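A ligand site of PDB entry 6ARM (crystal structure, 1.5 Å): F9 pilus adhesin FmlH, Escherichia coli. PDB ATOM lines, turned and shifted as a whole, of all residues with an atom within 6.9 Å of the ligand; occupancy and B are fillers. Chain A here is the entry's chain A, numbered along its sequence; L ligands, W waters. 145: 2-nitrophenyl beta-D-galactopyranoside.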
ATOM      1  N   PHE A   1      18.073   8.478   2.155  1.00  0.00           N
ATOM      2  CA  PHE A   1      18.822   9.731   2.209  1.00  0.00           C
ATOM      3  C   PHE A   1      18.049  10.843   1.533  1.00  0.00           C
ATOM      4  O   PHE A   1      17.490  10.635   0.446  1.00  0.00           O
ATOM      5  CB  PHE A   1      20.199   9.538   1.566  1.00  0.00           C
ATOM      6  CG  PHE A   1      21.022  10.801   1.482  1.00  0.00           C
ATOM      7  CD1 PHE A   1      21.127  11.496   0.289  1.00  0.00           C
ATOM      8  CD2 PHE A   1      21.712  11.280   2.595  1.00  0.00           C
ATOM      9  CE1 PHE A   1      21.885  12.655   0.202  1.00  0.00           C
ATOM     10  CE2 PHE A   1      22.474  12.447   2.506  1.00  0.00           C
ATOM     11  CZ  PHE A   1      22.554  13.131   1.308  1.00  0.00           C
ATOM     12  N   SER A   2      18.012  12.012   2.166  1.00  0.00           N
ATOM     13  CA  SER A   2      17.227  13.148   1.673  1.00  0.00           C
ATOM     14  C   SER A   2      17.958  14.466   1.924  1.00  0.00           C
ATOM     15  O   SER A   2      18.705  14.605   2.897  1.00  0.00           O
ATOM     16  CB  SER A   2      15.848  13.197   2.345  1.00  0.00           C
ATOM     17  OG  SER A   2      15.135  11.988   2.157  1.00  0.00           O
ATOM     18  N   SER A  10      11.490  17.756   0.810  1.00  0.00           N
ATOM     19  CA  SER A  10      12.575  16.788   0.708  1.00  0.00           C
ATOM     20  C   SER A  10      12.899  16.441  -0.736  1.00  0.00           C
ATOM     21  O   SER A  10      12.019  16.389  -1.591  1.00  0.00           O
ATOM     22  CB  SER A  10      12.232  15.510   1.466  1.00  0.00           C
ATOM     23  OG  SER A  10      12.036  15.795   2.838  1.00  0.00           O
ATOM     24  N   ILE A  11      14.190  16.177  -0.973  1.00  0.00           N
ATOM     25  CA  ILE A  11      14.727  15.826  -2.280  1.00  0.00           C
ATOM     26  C   ILE A  11      15.519  14.515  -2.186  1.00  0.00           C
ATOM     27  O   ILE A  11      16.400  14.359  -1.330  1.00  0.00           O
ATOM     28  CB  ILE A  11      15.643  16.939  -2.809  1.00  0.00           C
ATOM     29  CG1 ILE A  11      14.931  18.291  -2.678  1.00  0.00           C
ATOM     30  CG2 ILE A  11      16.060  16.633  -4.256  1.00  0.00           C
ATOM     31  CD1 ILE A  11      15.813  19.501  -2.959  1.00  0.00           C
ATOM     32  N   GLY A  12      15.196  13.577  -3.071  1.00  0.00           N
ATOM     33  CA  GLY A  12      15.815  12.270  -3.015  1.00  0.00           C
ATOM     34  C   GLY A  12      16.802  12.004  -4.151  1.00  0.00           C
ATOM     35  O   GLY A  12      17.579  11.066  -4.089  1.00  0.00           O
ATOM     36  N   TRP A  43      20.129  14.608   5.312  1.00  0.00           N
ATOM     37  CA  TRP A  43      20.040  13.791   6.518  1.00  0.00           C
ATOM     38  C   TRP A  43      19.835  12.321   6.189  1.00  0.00           C
ATOM     39  O   TRP A  43      19.469  11.968   5.072  1.00  0.00           O
ATOM     40  CB  TRP A  43      18.899  14.299   7.435  1.00  0.00           C
ATOM     41  CG  TRP A  43      17.572  14.328   6.744  1.00  0.00           C
ATOM     42  CD1 TRP A  43      16.630  13.336   6.716  1.00  0.00           C
ATOM     43  CD2 TRP A  43      17.053  15.389   5.938  1.00  0.00           C
ATOM     44  NE1 TRP A  43      15.560  13.722   5.960  1.00  0.00           N
ATOM     45  CE2 TRP A  43      15.791  14.979   5.459  1.00  0.00           C
ATOM     46  CE3 TRP A  43      17.547  16.652   5.577  1.00  0.00           C
ATOM     47  CZ2 TRP A  43      15.007  15.785   4.633  1.00  0.00           C
ATOM     48  CZ3 TRP A  43      16.767  17.454   4.744  1.00  0.00           C
ATOM     49  CH2 TRP A  43      15.520  17.017   4.283  1.00  0.00           C
ATOM     50  N   ASN A  44      20.069  11.481   7.189  1.00  0.00           N
ATOM     51  CA  ASN A  44      19.832  10.063   7.116  1.00  0.00           C
ATOM     52  C   ASN A  44      18.349   9.818   7.408  1.00  0.00           C
ATOM     53  O   ASN A  44      17.810  10.412   8.348  1.00  0.00           O
ATOM     54  CB  ASN A  44      20.716   9.321   8.106  1.00  0.00           C
ATOM     55  CG  ASN A  44      20.627   7.831   7.962  1.00  0.00           C
ATOM     56  OD1 ASN A  44      19.629   7.222   8.373  1.00  0.00           O
ATOM     57  ND2 ASN A  44      21.674   7.230   7.388  1.00  0.00           N
ATOM     58  N   ASP A  45      17.685   8.991   6.614  1.00  0.00           N
ATOM     59  CA  ASP A  45      16.229   8.902   6.742  1.00  0.00           C
ATOM     60  C   ASP A  45      15.786   7.940   7.843  1.00  0.00           C
ATOM     61  O   ASP A  45      14.601   7.846   8.133  1.00  0.00           O
ATOM     62  CB  ASP A  45      15.608   8.531   5.398  1.00  0.00           C
ATOM     63  CG  ASP A  45      15.357   9.744   4.517  1.00  0.00           C
ATOM     64  OD1 ASP A  45      14.731  10.721   4.992  1.00  0.00           O
ATOM     65  OD2 ASP A  45      15.806   9.751   3.353  1.00  0.00           O
ATOM     66  N   TYR A  46      16.737   7.268   8.479  1.00  0.00           N
ATOM     67  CA  TYR A  46      16.450   6.490   9.692  1.00  0.00           C
ATOM     68  C   TYR A  46      17.001   7.132  10.944  1.00  0.00           C
ATOM     69  O   TYR A  46      16.360   7.123  11.994  1.00  0.00           O
ATOM     70  CB  TYR A  46      17.032   5.080   9.614  1.00  0.00           C
ATOM     71  CG  TYR A  46      16.683   4.350   8.356  1.00  0.00           C
ATOM     72  CD1 TYR A  46      15.422   4.444   7.804  1.00  0.00           C
ATOM     73  CD2 TYR A  46      17.633   3.567   7.718  1.00  0.00           C
ATOM     74  CE1 TYR A  46      15.107   3.788   6.644  1.00  0.00           C
ATOM     75  CE2 TYR A  46      17.337   2.904   6.580  1.00  0.00           C
ATOM     76  CZ  TYR A  46      16.078   3.011   6.035  1.00  0.00           C
ATOM     77  OH  TYR A  46      15.793   2.337   4.872  1.00  0.00           O
ATOM     78  N   GLY A  47      18.219   7.653  10.828  1.00  0.00           N
ATOM     79  CA  GLY A  47      18.959   8.125  11.977  1.00  0.00           C
ATOM     80  C   GLY A  47      19.630   6.959  12.683  1.00  0.00           C
ATOM     81  O   GLY A  47      19.512   5.813  12.245  1.00  0.00           O
ATOM     82  N   ASP A  51      21.854   2.597   8.703  1.00  0.00           N
ATOM     83  CA  ASP A  51      22.235   2.456   7.285  1.00  0.00           C
ATOM     84  C   ASP A  51      22.906   3.768   6.847  1.00  0.00           C
ATOM     85  O   ASP A  51      22.250   4.641   6.267  1.00  0.00           O
ATOM     86  CB  ASP A  51      21.008   2.149   6.422  1.00  0.00           C
ATOM     87  CG  ASP A  51      21.365   1.854   4.981  1.00  0.00           C
ATOM     88  OD1 ASP A  51      22.564   1.696   4.681  1.00  0.00           O
ATOM     89  OD2 ASP A  51      20.416   1.742   4.158  1.00  0.00           O
ATOM     90  N   THR A  52      24.184   3.904   7.174  1.00  0.00           N
ATOM     91  CA  THR A  52      24.879   5.187   7.028  1.00  0.00           C
ATOM     92  C   THR A  52      25.028   5.589   5.563  1.00  0.00           C
ATOM     93  O   THR A  52      25.353   4.762   4.721  1.00  0.00           O
ATOM     94  CB  THR A  52      26.282   5.136   7.702  1.00  0.00           C
ATOM     95  OG1 THR A  52      26.115   4.903   9.107  1.00  0.00           O
ATOM     96  CG2 THR A  52      27.043   6.449   7.487  1.00  0.00           C
ATOM     97  N   ASP A  53      24.755   6.866   5.278  1.00  0.00           N
ATOM     98  CA  ASP A  53      24.935   7.416   3.923  1.00  0.00           C
ATOM     99  C   ASP A  53      26.331   7.965   3.693  1.00  0.00           C
ATOM    100  O   ASP A  53      26.950   8.518   4.604  1.00  0.00           O
ATOM    101  CB  ASP A  53      23.917   8.519   3.653  1.00  0.00           C
ATOM    102  CG  ASP A  53      22.488   8.010   3.676  1.00  0.00           C
ATOM    103  OD1 ASP A  53      22.219   7.012   2.969  1.00  0.00           O
ATOM    104  OD2 ASP A  53      21.653   8.579   4.411  1.00  0.00           O
ATOM    105  N   ILE A  94      26.870  10.541   6.617  1.00  0.00           N
ATOM    106  CA  ILE A  94      25.622  11.094   7.165  1.00  0.00           C
ATOM    107  C   ILE A  94      24.787   9.969   7.779  1.00  0.00           C
ATOM    108  O   ILE A  94      24.344   9.053   7.069  1.00  0.00           O
ATOM    109  CB  ILE A  94      24.816  11.818   6.074  1.00  0.00           C
ATOM    110  CG1 ILE A  94      25.594  13.020   5.507  1.00  0.00           C
ATOM    111  CG2 ILE A  94      23.431  12.244   6.599  1.00  0.00           C
ATOM    112  CD1 ILE A  94      25.704  14.165   6.434  1.00  0.00           C
ATOM    113  N   LYS A 132      25.468   9.878  -3.819  1.00  0.00           N
ATOM    114  CA  LYS A 132      25.121   9.221  -2.568  1.00  0.00           C
ATOM    115  C   LYS A 132      25.145   7.713  -2.727  1.00  0.00           C
ATOM    116  O   LYS A 132      24.602   7.176  -3.694  1.00  0.00           O
ATOM    117  CB  LYS A 132      23.740   9.659  -2.082  1.00  0.00           C
ATOM    118  CG  LYS A 132      23.149   8.753  -0.984  1.00  0.00           C
ATOM    119  CD  LYS A 132      22.094   7.796  -1.543  1.00  0.00           C
ATOM    120  CE  LYS A 132      21.737   6.743  -0.483  1.00  0.00           C
ATOM    121  NZ  LYS A 132      20.519   5.948  -0.865  1.00  0.00           N
ATOM    122  N   ILE A 133      25.765   7.024  -1.776  1.00  0.00           N
ATOM    123  CA  ILE A 133      25.582   5.584  -1.664  1.00  0.00           C
ATOM    124  C   ILE A 133      25.553   5.238  -0.175  1.00  0.00           C
ATOM    125  O   ILE A 133      26.308   5.795   0.614  1.00  0.00           O
ATOM    126  CB  ILE A 133      26.683   4.798  -2.415  1.00  0.00           C
ATOM    127  CG1 ILE A 133      26.338   3.301  -2.485  1.00  0.00           C
ATOM    128  CG2 ILE A 133      28.059   5.027  -1.795  1.00  0.00           C
ATOM    129  CD1 ILE A 133      27.148   2.534  -3.540  1.00  0.00           C
ATOM    130  N   ALA A 134      24.630   4.365   0.220  1.00  0.00           N
ATOM    131  CA  ALA A 134      24.506   3.993   1.623  1.00  0.00           C
ATOM    132  C   ALA A 134      25.339   2.758   1.947  1.00  0.00           C
ATOM    133  O   ALA A 134      26.329   2.479   1.275  1.00  0.00           O
ATOM    134  CB  ALA A 134      23.037   3.790   1.984  1.00  0.00           C
ATOM    135  N   THR A 135      24.934   2.013   2.967  1.00  0.00           N
ATOM    136  CA  THR A 135      25.779   0.981   3.555  1.00  0.00           C
ATOM    137  C   THR A 135      25.223  -0.447   3.390  1.00  0.00           C
ATOM    138  O   THR A 135      25.977  -1.385   3.138  1.00  0.00           O
ATOM    139  CB  THR A 135      25.988   1.253   5.066  1.00  0.00           C
ATOM    140  OG1 THR A 135      26.656   2.519   5.245  1.00  0.00           O
ATOM    141  CG2 THR A 135      26.811   0.158   5.732  1.00  0.00           C
ATOM    142  N   LEU A 136      23.903  -0.584   3.526  1.00  0.00           N
ATOM    143  CA  LEU A 136      23.247  -1.893   3.442  1.00  0.00           C
ATOM    144  C   LEU A 136      22.771  -2.210   2.017  1.00  0.00           C
ATOM    145  O   LEU A 136      22.447  -1.315   1.248  1.00  0.00           O
ATOM    146  CB  LEU A 136      22.058  -1.951   4.405  1.00  0.00           C
ATOM    147  CG  LEU A 136      22.306  -1.639   5.879  1.00  0.00           C
ATOM    148  CD1 LEU A 136      20.989  -1.514   6.624  1.00  0.00           C
ATOM    149  CD2 LEU A 136      23.220  -2.668   6.541  1.00  0.00           C
ATOM    150  N   GLY A 139      23.282  -0.277  -1.517  1.00  0.00           N
ATOM    151  CA  GLY A 139      23.604   1.077  -1.111  1.00  0.00           C
ATOM    152  C   GLY A 139      22.654   2.057  -1.766  1.00  0.00           C
ATOM    153  O   GLY A 139      22.649   3.236  -1.429  1.00  0.00           O
ATOM    154  N   ASN A 140      21.865   1.562  -2.726  1.00  0.00           N
ATOM    155  CA  ASN A 140      20.819   2.373  -3.334  1.00  0.00           C
ATOM    156  C   ASN A 140      21.358   3.738  -3.803  1.00  0.00           C
ATOM    157  O   ASN A 140      20.913   4.793  -3.371  1.00  0.00           O
ATOM    158  CB  ASN A 140      19.686   2.542  -2.309  1.00  0.00           C
ATOM    159  CG  ASN A 140      18.555   3.387  -2.815  1.00  0.00           C
ATOM    160  OD1 ASN A 140      18.277   3.431  -4.016  1.00  0.00           O
ATOM    161  ND2 ASN A 140      17.892   4.088  -1.905  1.00  0.00           N
ATOM    162  N   PRO A 141      22.366   3.701  -4.693  1.00  0.00           N
ATOM    163  CA  PRO A 141      23.053   4.932  -5.088  1.00  0.00           C
ATOM    164  C   PRO A 141      22.136   5.890  -5.814  1.00  0.00           C
ATOM    165  O   PRO A 141      21.277   5.463  -6.588  1.00  0.00           O
ATOM    166  CB  PRO A 141      24.156   4.428  -6.023  1.00  0.00           C
ATOM    167  CG  PRO A 141      23.622   3.136  -6.567  1.00  0.00           C
ATOM    168  CD  PRO A 141      22.899   2.525  -5.399  1.00  0.00           C
ATOM    169  N   ARG A 142      22.325   7.177  -5.562  1.00  0.00           N
ATOM    170  CA  ARG A 142      21.509   8.190  -6.212  1.00  0.00           C
ATOM    171  C   ARG A 142      22.363   9.397  -6.574  1.00  0.00           C
ATOM    172  O   ARG A 142      23.361   9.689  -5.917  1.00  0.00           O
ATOM    173  CB  ARG A 142      20.363   8.620  -5.298  1.00  0.00           C
ATOM    174  CG  ARG A 142      19.529   7.454  -4.758  1.00  0.00           C
ATOM    175  CD  ARG A 142      18.062   7.673  -5.042  1.00  0.00           C
ATOM    176  NE  ARG A 142      17.809   7.837  -6.472  1.00  0.00           N
ATOM    177  CZ  ARG A 142      16.623   8.151  -6.998  1.00  0.00           C
ATOM    178  NH1 ARG A 142      16.494   8.274  -8.313  1.00  0.00           N
ATOM    179  NH2 ARG A 142      15.572   8.327  -6.212  1.00  0.00           N
HETATM  180  C1  145 L   1      16.634   5.076   2.578  1.00  0.00           C
HETATM  181  C2  145 L   1      17.511   4.656   1.419  1.00  0.00           C
HETATM  182  O2  145 L   1      16.812   3.768   0.579  1.00  0.00           O
HETATM  183  C3  145 L   1      18.777   3.988   1.902  1.00  0.00           C
HETATM  184  O3  145 L   1      19.613   3.716   0.789  1.00  0.00           O
HETATM  185  C4  145 L   1      19.454   4.899   2.899  1.00  0.00           C
HETATM  186  O4  145 L   1      19.842   6.084   2.248  1.00  0.00           O
HETATM  187  C5  145 L   1      18.486   5.220   4.018  1.00  0.00           C
HETATM  188  C6  145 L   1      19.154   6.074   5.095  1.00  0.00           C
HETATM  189  O6  145 L   1      19.164   7.438   4.746  1.00  0.00           O
HETATM  190  O5  145 L   1      17.367   5.889   3.478  1.00  0.00           O
HETATM  191  O1  145 L   1      15.581   5.788   1.976  1.00  0.00           O
HETATM  192  C1' 145 L   1      14.524   6.197   2.808  1.00  0.00           C
HETATM  193  C2' 145 L   1      13.767   7.316   2.463  1.00  0.00           C
HETATM  194  C3' 145 L   1      12.718   7.710   3.293  1.00  0.00           C
HETATM  195  C4' 145 L   1      12.437   6.993   4.434  1.00  0.00           C
HETATM  196  C5' 145 L   1      13.178   5.881   4.770  1.00  0.00           C
HETATM  197  C6' 145 L   1      14.219   5.482   3.950  1.00  0.00           C
HETATM  198  N1' 145 L   1      14.032   8.097   1.310  1.00  0.00           N
HETATM  199  O2' 145 L   1      13.175   8.854   0.863  1.00  0.00           O
HETATM  200  O3' 145 L   1      15.116   8.065   0.731  1.00  0.00           O
HETATM  201  O   HOH W   1      20.843   1.201   1.580  1.00  0.00           O
HETATM  202  O   HOH W   2      18.243   7.488  -0.669  1.00  0.00           O
HETATM  203  O   HOH W   3      15.861   6.453  -1.519  1.00  0.00           O
HETATM  204  O   HOH W   4      14.152   4.344  -0.006  1.00  0.00           O
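An oxygen (O4) of the ligand is in hydrogen-bond range of the side-chain carboxylate of Asp 53, 2.7 Å away.
An oxygen (O2) of the ligand lies within hydrogen-bond range of the side-chain amide nitrogen of Asn 140.
The backbone NH (N) of Asp 45 lies within hydrogen-bond range of an oxygen (O6) of the ligand (2.8 Å).
The side-chain amino group (NZ) of Lys 132 lies within hydrogen-bond range of an oxygen (O3) of the ligand (2.9 Å).
The backbone NH (N) of Phe 1 is in hydrogen-bond range of an oxygen (O4) of the ligand.
N of Ile 94 sits at hydrogen-bond distance from O of Asp 53, 2.9 Å away.
OD2 of Asp 45 lies within hydrogen-bond range of N of Phe 1 (2.9 Å).
The side-chain carboxylate (OD1) of Asp 45 lies within hydrogen-bond range of the indole nitrogen (NE1) of Trp 43 (3.3 Å).
The backbone carbonyl oxygen of Lys 132 sits at hydrogen-bond distance from the backbone NH of Arg 142 (2.9 Å).
ND2 of Asn 44 lies within hydrogen-bond range of O of Ile 94.
The side-chain carboxylate of Asp 51 sits at hydrogen-bond distance from the backbone NH of Thr 135, at 2.9 Å.
The backbone carbonyl oxygen (O) of Gly 139 is in hydrogen-bond range of the backbone NH (N) of Ala 134 (2.8 Å).
N of Trp 43 is in hydrogen-bond range of O of Ser 2 (2.8 Å).
Water W3 bridges an oxygen (O3') of the ligand (2.9 Å) and the side-chain amide nitrogen of Asn 140 (3.1 Å).
Water W1 lies within hydrogen-bond range of the side-chain carboxylate (OD2) of Asp 51 (2.7 Å), an oxygen (O3) of the ligand (2.9 Å) and the backbone carbonyl oxygen (O) of Leu 136 (3.0 Å).
Water W2 lies within hydrogen-bond range of NZ of Lys 132 (2.8 Å), N of Phe 1 (3.0 Å) and O3' of the ligand (3.5 Å).
Merely in contact with the ligand: Ser 2 (3.9 Å), Asn 44 (3.5 Å), Tyr 46 (3.3 Å), Asp 51 (3.5 Å), Ala 134 (3.6 Å) and Gly 139 (3.8 Å).
Of the 23 residues printed, 11 come within 4 Å of the ligand.
The nearest printed residue that does not touch the ligand is Trp 43 (4.6 Å).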
